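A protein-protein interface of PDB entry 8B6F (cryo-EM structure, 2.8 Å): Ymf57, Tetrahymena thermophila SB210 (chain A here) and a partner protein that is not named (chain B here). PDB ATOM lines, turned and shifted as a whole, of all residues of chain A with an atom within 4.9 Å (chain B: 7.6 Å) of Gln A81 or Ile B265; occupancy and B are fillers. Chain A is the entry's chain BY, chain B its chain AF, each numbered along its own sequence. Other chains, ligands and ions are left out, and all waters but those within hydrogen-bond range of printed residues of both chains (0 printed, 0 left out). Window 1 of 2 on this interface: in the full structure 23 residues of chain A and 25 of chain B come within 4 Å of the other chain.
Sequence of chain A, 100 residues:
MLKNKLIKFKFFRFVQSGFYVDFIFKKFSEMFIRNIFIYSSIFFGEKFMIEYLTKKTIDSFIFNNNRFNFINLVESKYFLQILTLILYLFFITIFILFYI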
ATOM      1  N   SER A  76      17.392 -12.929   6.809  1.00  0.00           N
ATOM      2  CA  SER A  76      18.076 -11.862   7.533  1.00  0.00           C
ATOM      3  C   SER A  76      18.111 -10.583   6.709  1.00  0.00           C
ATOM      4  O   SER A  76      17.808  -9.496   7.213  1.00  0.00           O
ATOM      5  CB  SER A  76      19.493 -12.306   7.894  1.00  0.00           C
ATOM      6  OG  SER A  76      19.478 -13.538   8.592  1.00  0.00           O
ATOM      7  N   LYS A  77      18.485 -10.693   5.434  1.00  0.00           N
ATOM      8  CA  LYS A  77      18.512  -9.521   4.564  1.00  0.00           C
ATOM      9  C   LYS A  77      17.119  -8.934   4.397  1.00  0.00           C
ATOM     10  O   LYS A  77      16.949  -7.710   4.404  1.00  0.00           O
ATOM     11  CB  LYS A  77      19.099  -9.895   3.204  1.00  0.00           C
ATOM     12  CG  LYS A  77      20.587 -10.212   3.233  1.00  0.00           C
ATOM     13  CD  LYS A  77      21.425  -8.964   3.452  1.00  0.00           C
ATOM     14  CE  LYS A  77      22.910  -9.279   3.361  1.00  0.00           C
ATOM     15  NZ  LYS A  77      23.746  -8.054   3.491  1.00  0.00           N
ATOM     16  N   TYR A  78      16.109  -9.790   4.239  1.00  0.00           N
ATOM     17  CA  TYR A  78      14.743  -9.305   4.080  1.00  0.00           C
ATOM     18  C   TYR A  78      14.325  -8.450   5.271  1.00  0.00           C
ATOM     19  O   TYR A  78      13.870  -7.313   5.104  1.00  0.00           O
ATOM     20  CB  TYR A  78      13.802 -10.498   3.899  1.00  0.00           C
ATOM     21  CG  TYR A  78      12.332 -10.167   3.970  1.00  0.00           C
ATOM     22  CD1 TYR A  78      11.692  -9.516   2.924  1.00  0.00           C
ATOM     23  CD2 TYR A  78      11.572 -10.545   5.068  1.00  0.00           C
ATOM     24  CE1 TYR A  78      10.345  -9.225   2.982  1.00  0.00           C
ATOM     25  CE2 TYR A  78      10.225 -10.260   5.134  1.00  0.00           C
ATOM     26  CZ  TYR A  78       9.617  -9.602   4.088  1.00  0.00           C
ATOM     27  OH  TYR A  78       8.275  -9.316   4.151  1.00  0.00           O
ATOM     28  N   PHE A  79      14.467  -8.983   6.486  1.00  0.00           N
ATOM     29  CA  PHE A  79      14.056  -8.237   7.670  1.00  0.00           C
ATOM     30  C   PHE A  79      14.899  -6.982   7.865  1.00  0.00           C
ATOM     31  O   PHE A  79      14.373  -5.920   8.213  1.00  0.00           O
ATOM     32  CB  PHE A  79      14.131  -9.130   8.907  1.00  0.00           C
ATOM     33  CG  PHE A  79      13.010 -10.121   8.998  1.00  0.00           C
ATOM     34  CD1 PHE A  79      11.750  -9.718   9.405  1.00  0.00           C
ATOM     35  CD2 PHE A  79      13.210 -11.450   8.680  1.00  0.00           C
ATOM     36  CE1 PHE A  79      10.714 -10.622   9.491  1.00  0.00           C
ATOM     37  CE2 PHE A  79      12.177 -12.360   8.764  1.00  0.00           C
ATOM     38  CZ  PHE A  79      10.926 -11.943   9.169  1.00  0.00           C
ATOM     39  N   LEU A  80      16.211  -7.087   7.643  1.00  0.00           N
ATOM     40  CA  LEU A  80      17.090  -5.938   7.841  1.00  0.00           C
ATOM     41  C   LEU A  80      16.777  -4.823   6.853  1.00  0.00           C
ATOM     42  O   LEU A  80      16.814  -3.641   7.213  1.00  0.00           O
ATOM     43  CB  LEU A  80      18.554  -6.364   7.718  1.00  0.00           C
ATOM     44  CG  LEU A  80      19.589  -5.276   8.024  1.00  0.00           C
ATOM     45  CD1 LEU A  80      19.414  -4.722   9.432  1.00  0.00           C
ATOM     46  CD2 LEU A  80      20.999  -5.811   7.837  1.00  0.00           C
ATOM     47  N   GLN A  81      16.476  -5.174   5.603  1.00  0.00           N
ATOM     48  CA  GLN A  81      16.103  -4.154   4.628  1.00  0.00           C
ATOM     49  C   GLN A  81      14.795  -3.477   5.013  1.00  0.00           C
ATOM     50  O   GLN A  81      14.660  -2.256   4.879  1.00  0.00           O
ATOM     51  CB  GLN A  81      15.994  -4.771   3.234  1.00  0.00           C
ATOM     52  CG  GLN A  81      17.331  -5.158   2.633  1.00  0.00           C
ATOM     53  CD  GLN A  81      17.187  -5.787   1.265  1.00  0.00           C
ATOM     54  OE1 GLN A  81      16.111  -5.766   0.670  1.00  0.00           O
ATOM     55  NE2 GLN A  81      18.275  -6.354   0.757  1.00  0.00           N
ATOM     56  N   ILE A  82      13.815  -4.248   5.483  1.00  0.00           N
ATOM     57  CA  ILE A  82      12.551  -3.649   5.905  1.00  0.00           C
ATOM     58  C   ILE A  82      12.791  -2.668   7.045  1.00  0.00           C
ATOM     59  O   ILE A  82      12.284  -1.541   7.036  1.00  0.00           O
ATOM     60  CB  ILE A  82      11.543  -4.747   6.296  1.00  0.00           C
ATOM     61  CG1 ILE A  82      10.913  -5.342   5.035  1.00  0.00           C
ATOM     62  CG2 ILE A  82      10.463  -4.199   7.232  1.00  0.00           C
ATOM     63  CD1 ILE A  82      10.014  -6.529   5.285  1.00  0.00           C
ATOM     64  N   LEU A  83      13.569  -3.082   8.048  1.00  0.00           N
ATOM     65  CA  LEU A  83      13.830  -2.202   9.182  1.00  0.00           C
ATOM     66  C   LEU A  83      14.623  -0.977   8.753  1.00  0.00           C
ATOM     67  O   LEU A  83      14.359   0.135   9.222  1.00  0.00           O
ATOM     68  CB  LEU A  83      14.570  -2.956  10.285  1.00  0.00           C
ATOM     69  CG  LEU A  83      14.873  -2.136  11.543  1.00  0.00           C
ATOM     70  CD1 LEU A  83      13.586  -1.674  12.208  1.00  0.00           C
ATOM     71  CD2 LEU A  83      15.720  -2.929  12.521  1.00  0.00           C
ATOM     72  N   THR A  84      15.604  -1.161   7.869  1.00  0.00           N
ATOM     73  CA  THR A  84      16.392  -0.028   7.400  1.00  0.00           C
ATOM     74  C   THR A  84      15.506   0.986   6.693  1.00  0.00           C
ATOM     75  O   THR A  84      15.616   2.194   6.925  1.00  0.00           O
ATOM     76  CB  THR A  84      17.506  -0.512   6.470  1.00  0.00           C
ATOM     77  OG1 THR A  84      18.309  -1.489   7.144  1.00  0.00           O
ATOM     78  CG2 THR A  84      18.389   0.647   6.039  1.00  0.00           C
ATOM     79  N   LEU A  85      14.624   0.512   5.812  1.00  0.00           N
ATOM     80  CA  LEU A  85      13.682   1.417   5.168  1.00  0.00           C
ATOM     81  C   LEU A  85      12.843   2.151   6.207  1.00  0.00           C
ATOM     82  O   LEU A  85      12.741   3.383   6.183  1.00  0.00           O
ATOM     83  CB  LEU A  85      12.793   0.638   4.199  1.00  0.00           C
ATOM     84  CG  LEU A  85      11.702   1.445   3.494  1.00  0.00           C
ATOM     85  CD1 LEU A  85      12.297   2.589   2.686  1.00  0.00           C
ATOM     86  CD2 LEU A  85      10.859   0.544   2.607  1.00  0.00           C
ATOM     87  N   SER B 199       5.398 -10.472   4.882  1.00  0.00           N
ATOM     88  CA  SER B 199       4.997  -9.222   4.251  1.00  0.00           C
ATOM     89  C   SER B 199       3.590  -8.833   4.672  1.00  0.00           C
ATOM     90  O   SER B 199       3.316  -7.662   4.954  1.00  0.00           O
ATOM     91  CB  SER B 199       5.102  -9.354   2.737  1.00  0.00           C
ATOM     92  OG  SER B 199       6.428  -9.693   2.392  1.00  0.00           O
ATOM     93  N   ILE B 254       4.848   3.088   3.757  1.00  0.00           N
ATOM     94  CA  ILE B 254       5.743   1.951   3.941  1.00  0.00           C
ATOM     95  C   ILE B 254       4.952   0.658   4.066  1.00  0.00           C
ATOM     96  O   ILE B 254       5.372  -0.388   3.561  1.00  0.00           O
ATOM     97  CB  ILE B 254       6.657   2.173   5.159  1.00  0.00           C
ATOM     98  CG1 ILE B 254       7.605   3.347   4.926  1.00  0.00           C
ATOM     99  CG2 ILE B 254       7.449   0.905   5.479  1.00  0.00           C
ATOM    100  CD1 ILE B 254       8.540   3.144   3.766  1.00  0.00           C
ATOM    101  N   ILE B 257       4.144  -0.179   0.618  1.00  0.00           N
ATOM    102  CA  ILE B 257       5.350  -0.587  -0.099  1.00  0.00           C
ATOM    103  C   ILE B 257       5.673  -2.042   0.214  1.00  0.00           C
ATOM    104  O   ILE B 257       5.967  -2.840  -0.683  1.00  0.00           O
ATOM    105  CB  ILE B 257       6.529   0.340   0.260  1.00  0.00           C
ATOM    106  CG1 ILE B 257       6.332   1.742  -0.331  1.00  0.00           C
ATOM    107  CG2 ILE B 257       7.859  -0.269  -0.199  1.00  0.00           C
ATOM    108  CD1 ILE B 257       6.698   1.880  -1.793  1.00  0.00           C
ATOM    109  N   ILE B 258       5.627  -2.405   1.496  1.00  0.00           N
ATOM    110  CA  ILE B 258       5.899  -3.785   1.886  1.00  0.00           C
ATOM    111  C   ILE B 258       4.833  -4.711   1.320  1.00  0.00           C
ATOM    112  O   ILE B 258       5.129  -5.829   0.881  1.00  0.00           O
ATOM    113  CB  ILE B 258       6.000  -3.896   3.419  1.00  0.00           C
ATOM    114  CG1 ILE B 258       7.179  -3.062   3.928  1.00  0.00           C
ATOM    115  CG2 ILE B 258       6.160  -5.354   3.841  1.00  0.00           C
ATOM    116  CD1 ILE B 258       7.246  -2.937   5.434  1.00  0.00           C
ATOM    117  N   LYS B 259       3.575  -4.266   1.325  1.00  0.00           N
ATOM    118  CA  LYS B 259       2.493  -5.099   0.810  1.00  0.00           C
ATOM    119  C   LYS B 259       2.681  -5.397  -0.671  1.00  0.00           C
ATOM    120  O   LYS B 259       2.631  -6.556  -1.095  1.00  0.00           O
ATOM    121  CB  LYS B 259       1.148  -4.409   1.048  1.00  0.00           C
ATOM    122  CG  LYS B 259      -0.053  -5.254   0.656  1.00  0.00           C
ATOM    123  CD  LYS B 259      -0.188  -6.467   1.544  1.00  0.00           C
ATOM    124  CE  LYS B 259      -1.427  -7.264   1.213  1.00  0.00           C
ATOM    125  NZ  LYS B 259      -1.513  -8.455   2.094  1.00  0.00           N
ATOM    126  N   LEU B 260       2.907  -4.359  -1.473  1.00  0.00           N
ATOM    127  CA  LEU B 260       2.971  -4.544  -2.916  1.00  0.00           C
ATOM    128  C   LEU B 260       4.279  -5.197  -3.341  1.00  0.00           C
ATOM    129  O   LEU B 260       4.282  -6.085  -4.199  1.00  0.00           O
ATOM    130  CB  LEU B 260       2.788  -3.204  -3.621  1.00  0.00           C
ATOM    131  CG  LEU B 260       1.335  -2.782  -3.850  1.00  0.00           C
ATOM    132  CD1 LEU B 260       0.546  -2.771  -2.550  1.00  0.00           C
ATOM    133  CD2 LEU B 260       1.291  -1.419  -4.509  1.00  0.00           C
ATOM    134  N   GLY B 261       5.392  -4.778  -2.749  1.00  0.00           N
ATOM    135  CA  GLY B 261       6.694  -5.255  -3.164  1.00  0.00           C
ATOM    136  C   GLY B 261       7.345  -4.329  -4.168  1.00  0.00           C
ATOM    137  O   GLY B 261       7.803  -4.767  -5.226  1.00  0.00           O
ATOM    138  N   ILE B 262       7.383  -3.044  -3.846  1.00  0.00           N
ATOM    139  CA  ILE B 262       7.937  -2.042  -4.740  1.00  0.00           C
ATOM    140  C   ILE B 262       9.442  -1.957  -4.516  1.00  0.00           C
ATOM    141  O   ILE B 262       9.966  -2.378  -3.483  1.00  0.00           O
ATOM    142  CB  ILE B 262       7.215  -0.690  -4.533  1.00  0.00           C
ATOM    143  CG1 ILE B 262       5.739  -0.845  -4.920  1.00  0.00           C
ATOM    144  CG2 ILE B 262       7.847   0.428  -5.353  1.00  0.00           C
ATOM    145  CD1 ILE B 262       4.828   0.259  -4.441  1.00  0.00           C
ATOM    146  N   ALA B 263      10.144  -1.387  -5.501  1.00  0.00           N
ATOM    147  CA  ALA B 263      11.602  -1.485  -5.619  1.00  0.00           C
ATOM    148  C   ALA B 263      12.368  -1.490  -4.303  1.00  0.00           C
ATOM    149  O   ALA B 263      13.251  -2.344  -4.144  1.00  0.00           O
ATOM    150  CB  ALA B 263      12.103  -0.335  -6.502  1.00  0.00           C
ATOM    151  N   PRO B 264      12.119  -0.592  -3.349  1.00  0.00           N
ATOM    152  CA  PRO B 264      12.876  -0.676  -2.090  1.00  0.00           C
ATOM    153  C   PRO B 264      12.758  -2.037  -1.433  1.00  0.00           C
ATOM    154  O   PRO B 264      13.745  -2.545  -0.887  1.00  0.00           O
ATOM    155  CB  PRO B 264      12.258   0.440  -1.236  1.00  0.00           C
ATOM    156  CG  PRO B 264      11.676   1.390  -2.218  1.00  0.00           C
ATOM    157  CD  PRO B 264      11.196   0.555  -3.363  1.00  0.00           C
ATOM    158  N   ILE B 265      11.582  -2.651  -1.487  1.00  0.00           N
ATOM    159  CA  ILE B 265      11.350  -3.983  -0.933  1.00  0.00           C
ATOM    160  C   ILE B 265      10.816  -4.827  -2.085  1.00  0.00           C
ATOM    161  O   ILE B 265       9.613  -4.861  -2.350  1.00  0.00           O
ATOM    162  CB  ILE B 265      10.375  -3.962   0.246  1.00  0.00           C
ATOM    163  CG1 ILE B 265      10.786  -2.892   1.263  1.00  0.00           C
ATOM    164  CG2 ILE B 265      10.297  -5.336   0.896  1.00  0.00           C
ATOM    165  CD1 ILE B 265      12.135  -3.122   1.902  1.00  0.00           C
ATOM    166  N   GLN B 266      11.715  -5.529  -2.773  1.00  0.00           N
ATOM    167  CA  GLN B 266      11.364  -6.216  -4.010  1.00  0.00           C
ATOM    168  C   GLN B 266      11.839  -7.663  -4.023  1.00  0.00           C
ATOM    169  O   GLN B 266      11.243  -8.511  -4.692  1.00  0.00           O
ATOM    170  CB  GLN B 266      11.974  -5.480  -5.202  1.00  0.00           C
ATOM    171  CG  GLN B 266      13.480  -5.320  -5.083  1.00  0.00           C
ATOM    172  CD  GLN B 266      14.084  -4.602  -6.261  1.00  0.00           C
ATOM    173  OE1 GLN B 266      13.377  -3.985  -7.054  1.00  0.00           O
ATOM    174  NE2 GLN B 266      15.401  -4.685  -6.389  1.00  0.00           N
ATOM    175  N   LEU B 267      12.904  -7.955  -3.276  1.00  0.00           N
ATOM    176  CA  LEU B 267      13.534  -9.268  -3.367  1.00  0.00           C
ATOM    177  C   LEU B 267      12.578 -10.374  -2.940  1.00  0.00           C
ATOM    178  O   LEU B 267      12.585 -11.465  -3.520  1.00  0.00           O
ATOM    179  CB  LEU B 267      14.808  -9.293  -2.525  1.00  0.00           C
ATOM    180  CG  LEU B 267      15.821  -8.190  -2.843  1.00  0.00           C
ATOM    181  CD1 LEU B 267      17.043  -8.324  -1.958  1.00  0.00           C
ATOM    182  CD2 LEU B 267      16.223  -8.217  -4.311  1.00  0.00           C
ATOM    183  N   TYR B 268      11.746 -10.113  -1.933  1.00  0.00           N
ATOM    184  CA  TYR B 268      10.761 -11.108  -1.526  1.00  0.00           C
ATOM    185  C   TYR B 268       9.753 -11.359  -2.639  1.00  0.00           C
ATOM    186  O   TYR B 268       9.305 -12.494  -2.836  1.00  0.00           O
ATOM    187  CB  TYR B 268      10.055 -10.676  -0.241  1.00  0.00           C
ATOM    188  CG  TYR B 268       8.810  -9.850  -0.456  1.00  0.00           C
ATOM    189  CD1 TYR B 268       8.878  -8.467  -0.538  1.00  0.00           C
ATOM    190  CD2 TYR B 268       7.565 -10.454  -0.573  1.00  0.00           C
ATOM    191  CE1 TYR B 268       7.741  -7.710  -0.729  1.00  0.00           C
ATOM    192  CE2 TYR B 268       6.424  -9.705  -0.769  1.00  0.00           C
ATOM    193  CZ  TYR B 268       6.518  -8.334  -0.846  1.00  0.00           C
ATOM    194  OH  TYR B 268       5.381  -7.589  -1.037  1.00  0.00           O
ATOM    195  N   LYS B 269       9.390 -10.316  -3.384  1.00  0.00           N
ATOM    196  CA  LYS B 269       8.522 -10.503  -4.540  1.00  0.00           C
ATOM    197  C   LYS B 269       9.201 -11.372  -5.590  1.00  0.00           C
ATOM    198  O   LYS B 269       8.554 -12.214  -6.222  1.00  0.00           O
ATOM    199  CB  LYS B 269       8.137  -9.147  -5.128  1.00  0.00           C
ATOM    200  CG  LYS B 269       7.072  -9.220  -6.208  1.00  0.00           C
ATOM    201  CD  LYS B 269       6.720  -7.835  -6.721  1.00  0.00           C
ATOM    202  CE  LYS B 269       5.567  -7.878  -7.707  1.00  0.00           C
ATOM    203  NZ  LYS B 269       4.303  -8.340  -7.070  1.00  0.00           N
ATOM    204  N   ILE B 270      10.503 -11.177  -5.799  1.00  0.00           N
ATOM    205  CA  ILE B 270      11.235 -12.019  -6.740  1.00  0.00           C
ATOM    206  C   ILE B 270      11.181 -13.473  -6.293  1.00  0.00           C
ATOM    207  O   ILE B 270      10.957 -14.380  -7.103  1.00  0.00           O
ATOM    208  CB  ILE B 270      12.690 -11.531  -6.879  1.00  0.00           C
ATOM    209  CG1 ILE B 270      12.743 -10.040  -7.228  1.00  0.00           C
ATOM    210  CG2 ILE B 270      13.426 -12.342  -7.934  1.00  0.00           C
ATOM    211  CD1 ILE B 270      11.903  -9.639  -8.412  1.00  0.00           C
ATOM    212  N   ILE B 318      11.236   7.663  -2.519  1.00  0.00           N
ATOM    213  CA  ILE B 318      11.082   6.237  -2.792  1.00  0.00           C
ATOM    214  C   ILE B 318      11.379   5.942  -4.255  1.00  0.00           C
ATOM    215  O   ILE B 318      12.072   4.970  -4.578  1.00  0.00           O
ATOM    216  CB  ILE B 318       9.668   5.771  -2.392  1.00  0.00           C
ATOM    217  CG1 ILE B 318       9.502   5.787  -0.869  1.00  0.00           C
ATOM    218  CG2 ILE B 318       9.365   4.382  -2.955  1.00  0.00           C
ATOM    219  CD1 ILE B 318      10.405   4.822  -0.126  1.00  0.00           C
ATOM    220  N   GLY B 322      14.455   3.618  -5.459  1.00  0.00           N
ATOM    221  CA  GLY B 322      14.139   2.400  -6.185  1.00  0.00           C
ATOM    222  C   GLY B 322      14.780   2.352  -7.556  1.00  0.00           C
ATOM    223  O   GLY B 322      15.315   1.319  -7.963  1.00  0.00           O
ATOM    224  N   TYR B 325      18.416   1.732  -7.242  1.00  0.00           N
ATOM    225  CA  TYR B 325      18.697   0.409  -6.702  1.00  0.00           C
ATOM    226  C   TYR B 325      18.468  -0.691  -7.729  1.00  0.00           C
ATOM    227  O   TYR B 325      19.176  -1.704  -7.708  1.00  0.00           O
ATOM    228  CB  TYR B 325      17.832   0.161  -5.466  1.00  0.00           C
ATOM    229  CG  TYR B 325      18.098  -1.156  -4.776  1.00  0.00           C
ATOM    230  CD1 TYR B 325      19.339  -1.434  -4.219  1.00  0.00           C
ATOM    231  CD2 TYR B 325      17.099  -2.111  -4.659  1.00  0.00           C
ATOM    232  CE1 TYR B 325      19.582  -2.636  -3.581  1.00  0.00           C
ATOM    233  CE2 TYR B 325      17.331  -3.314  -4.024  1.00  0.00           C
ATOM    234  CZ  TYR B 325      18.574  -3.569  -3.485  1.00  0.00           C
ATOM    235  OH  TYR B 325      18.809  -4.767  -2.850  1.00  0.00           O
ATOM    236  N   ILE B 329      20.317  -4.113 -10.613  1.00  0.00           N
ATOM    237  CA  ILE B 329      19.815  -5.439 -10.269  1.00  0.00           C
ATOM    238  C   ILE B 329      19.079  -6.067 -11.447  1.00  0.00           C
ATOM    239  O   ILE B 329      19.193  -7.273 -11.689  1.00  0.00           O
ATOM    240  CB  ILE B 329      18.920  -5.354  -9.019  1.00  0.00           C
ATOM    241  CG1 ILE B 329      19.761  -4.939  -7.810  1.00  0.00           C
ATOM    242  CG2 ILE B 329      18.236  -6.688  -8.754  1.00  0.00           C
ATOM    243  CD1 ILE B 329      18.961  -4.667  -6.562  1.00  0.00           C
ATOM    244  N   ILE B 345       7.906  -4.640 -11.369  1.00  0.00           N
ATOM    245  CA  ILE B 345       8.501  -3.634 -10.493  1.00  0.00           C
ATOM    246  C   ILE B 345       8.823  -2.360 -11.264  1.00  0.00           C
ATOM    247  O   ILE B 345       8.568  -1.250 -10.783  1.00  0.00           O
ATOM    248  CB  ILE B 345       9.749  -4.214  -9.803  1.00  0.00           C
ATOM    249  CG1 ILE B 345       9.350  -5.343  -8.854  1.00  0.00           C
ATOM    250  CG2 ILE B 345      10.491  -3.133  -9.029  1.00  0.00           C
ATOM    251  CD1 ILE B 345      10.488  -6.259  -8.499  1.00  0.00           C
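Among the printed residues, merely in contact across the chains: Tyr A78 with Tyr B268 (3.5 Å), Gln A81 with Leu B267 (3.6 Å), Leu A85 with Ile B254 (3.6 Å), Leu A85 with Ile B265 (3.7 Å), Ile A82 with Ile B258 (3.9 Å), Gln A81 with Tyr B325 (3.98 Å) and Gln A81 with Ile B265 (3.999 Å).
Printed residues of chain A that touch a printed residue of chain B: Tyr A78, Gln A81, Ile A82 and Leu A85. Hydrophobic or aromatic side chains of chain A that line the printed part of chain B: Tyr A78, Ile A82 and Leu A85. Among the printed residues, 8 pairs touch across the chains. Among the printed residues, no Asp or Glu carboxylate lies within 4 Å of a Lys or Arg side-chain nitrogen of the other chain.
The side-chain hydroxyl of Tyr B268 lies within hydrogen-bond range of the backbone carbonyl oxygen of Ile B258 (2.6 Å). O of Lys B259 lies within hydrogen-bond range of OH of Tyr B268 (2.9 Å). OH of Tyr B268 sits at hydrogen-bond distance from N of Gly B261.
Of the printed residues of chain B, Gln A81 touches Ile B265, Leu B267 and Tyr B325. Of the printed residues of chain B, Leu A85 touches Ile B254 (3.6 Å) and Ile B265 (3.7 Å). Of the printed residues of chain A, Ile B254 touches Leu A85 (3.6 Å). Of the printed residues of chain A, Ile B265 touches Gln A81 (3.999 Å) and Leu A85 (3.7 Å). The nearest printed residue of chain B that does not touch Gln A81 is Pro B264 (4.3 Å). The nearest printed residue of chain B that does not touch Leu A85 is Ile B318 (4.1 Å).
The side-chain hydroxyl (OH) of Tyr A78 lies within hydrogen-bond range of the side-chain hydroxyl (OG) of Ser B199, at 2.6 Å.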
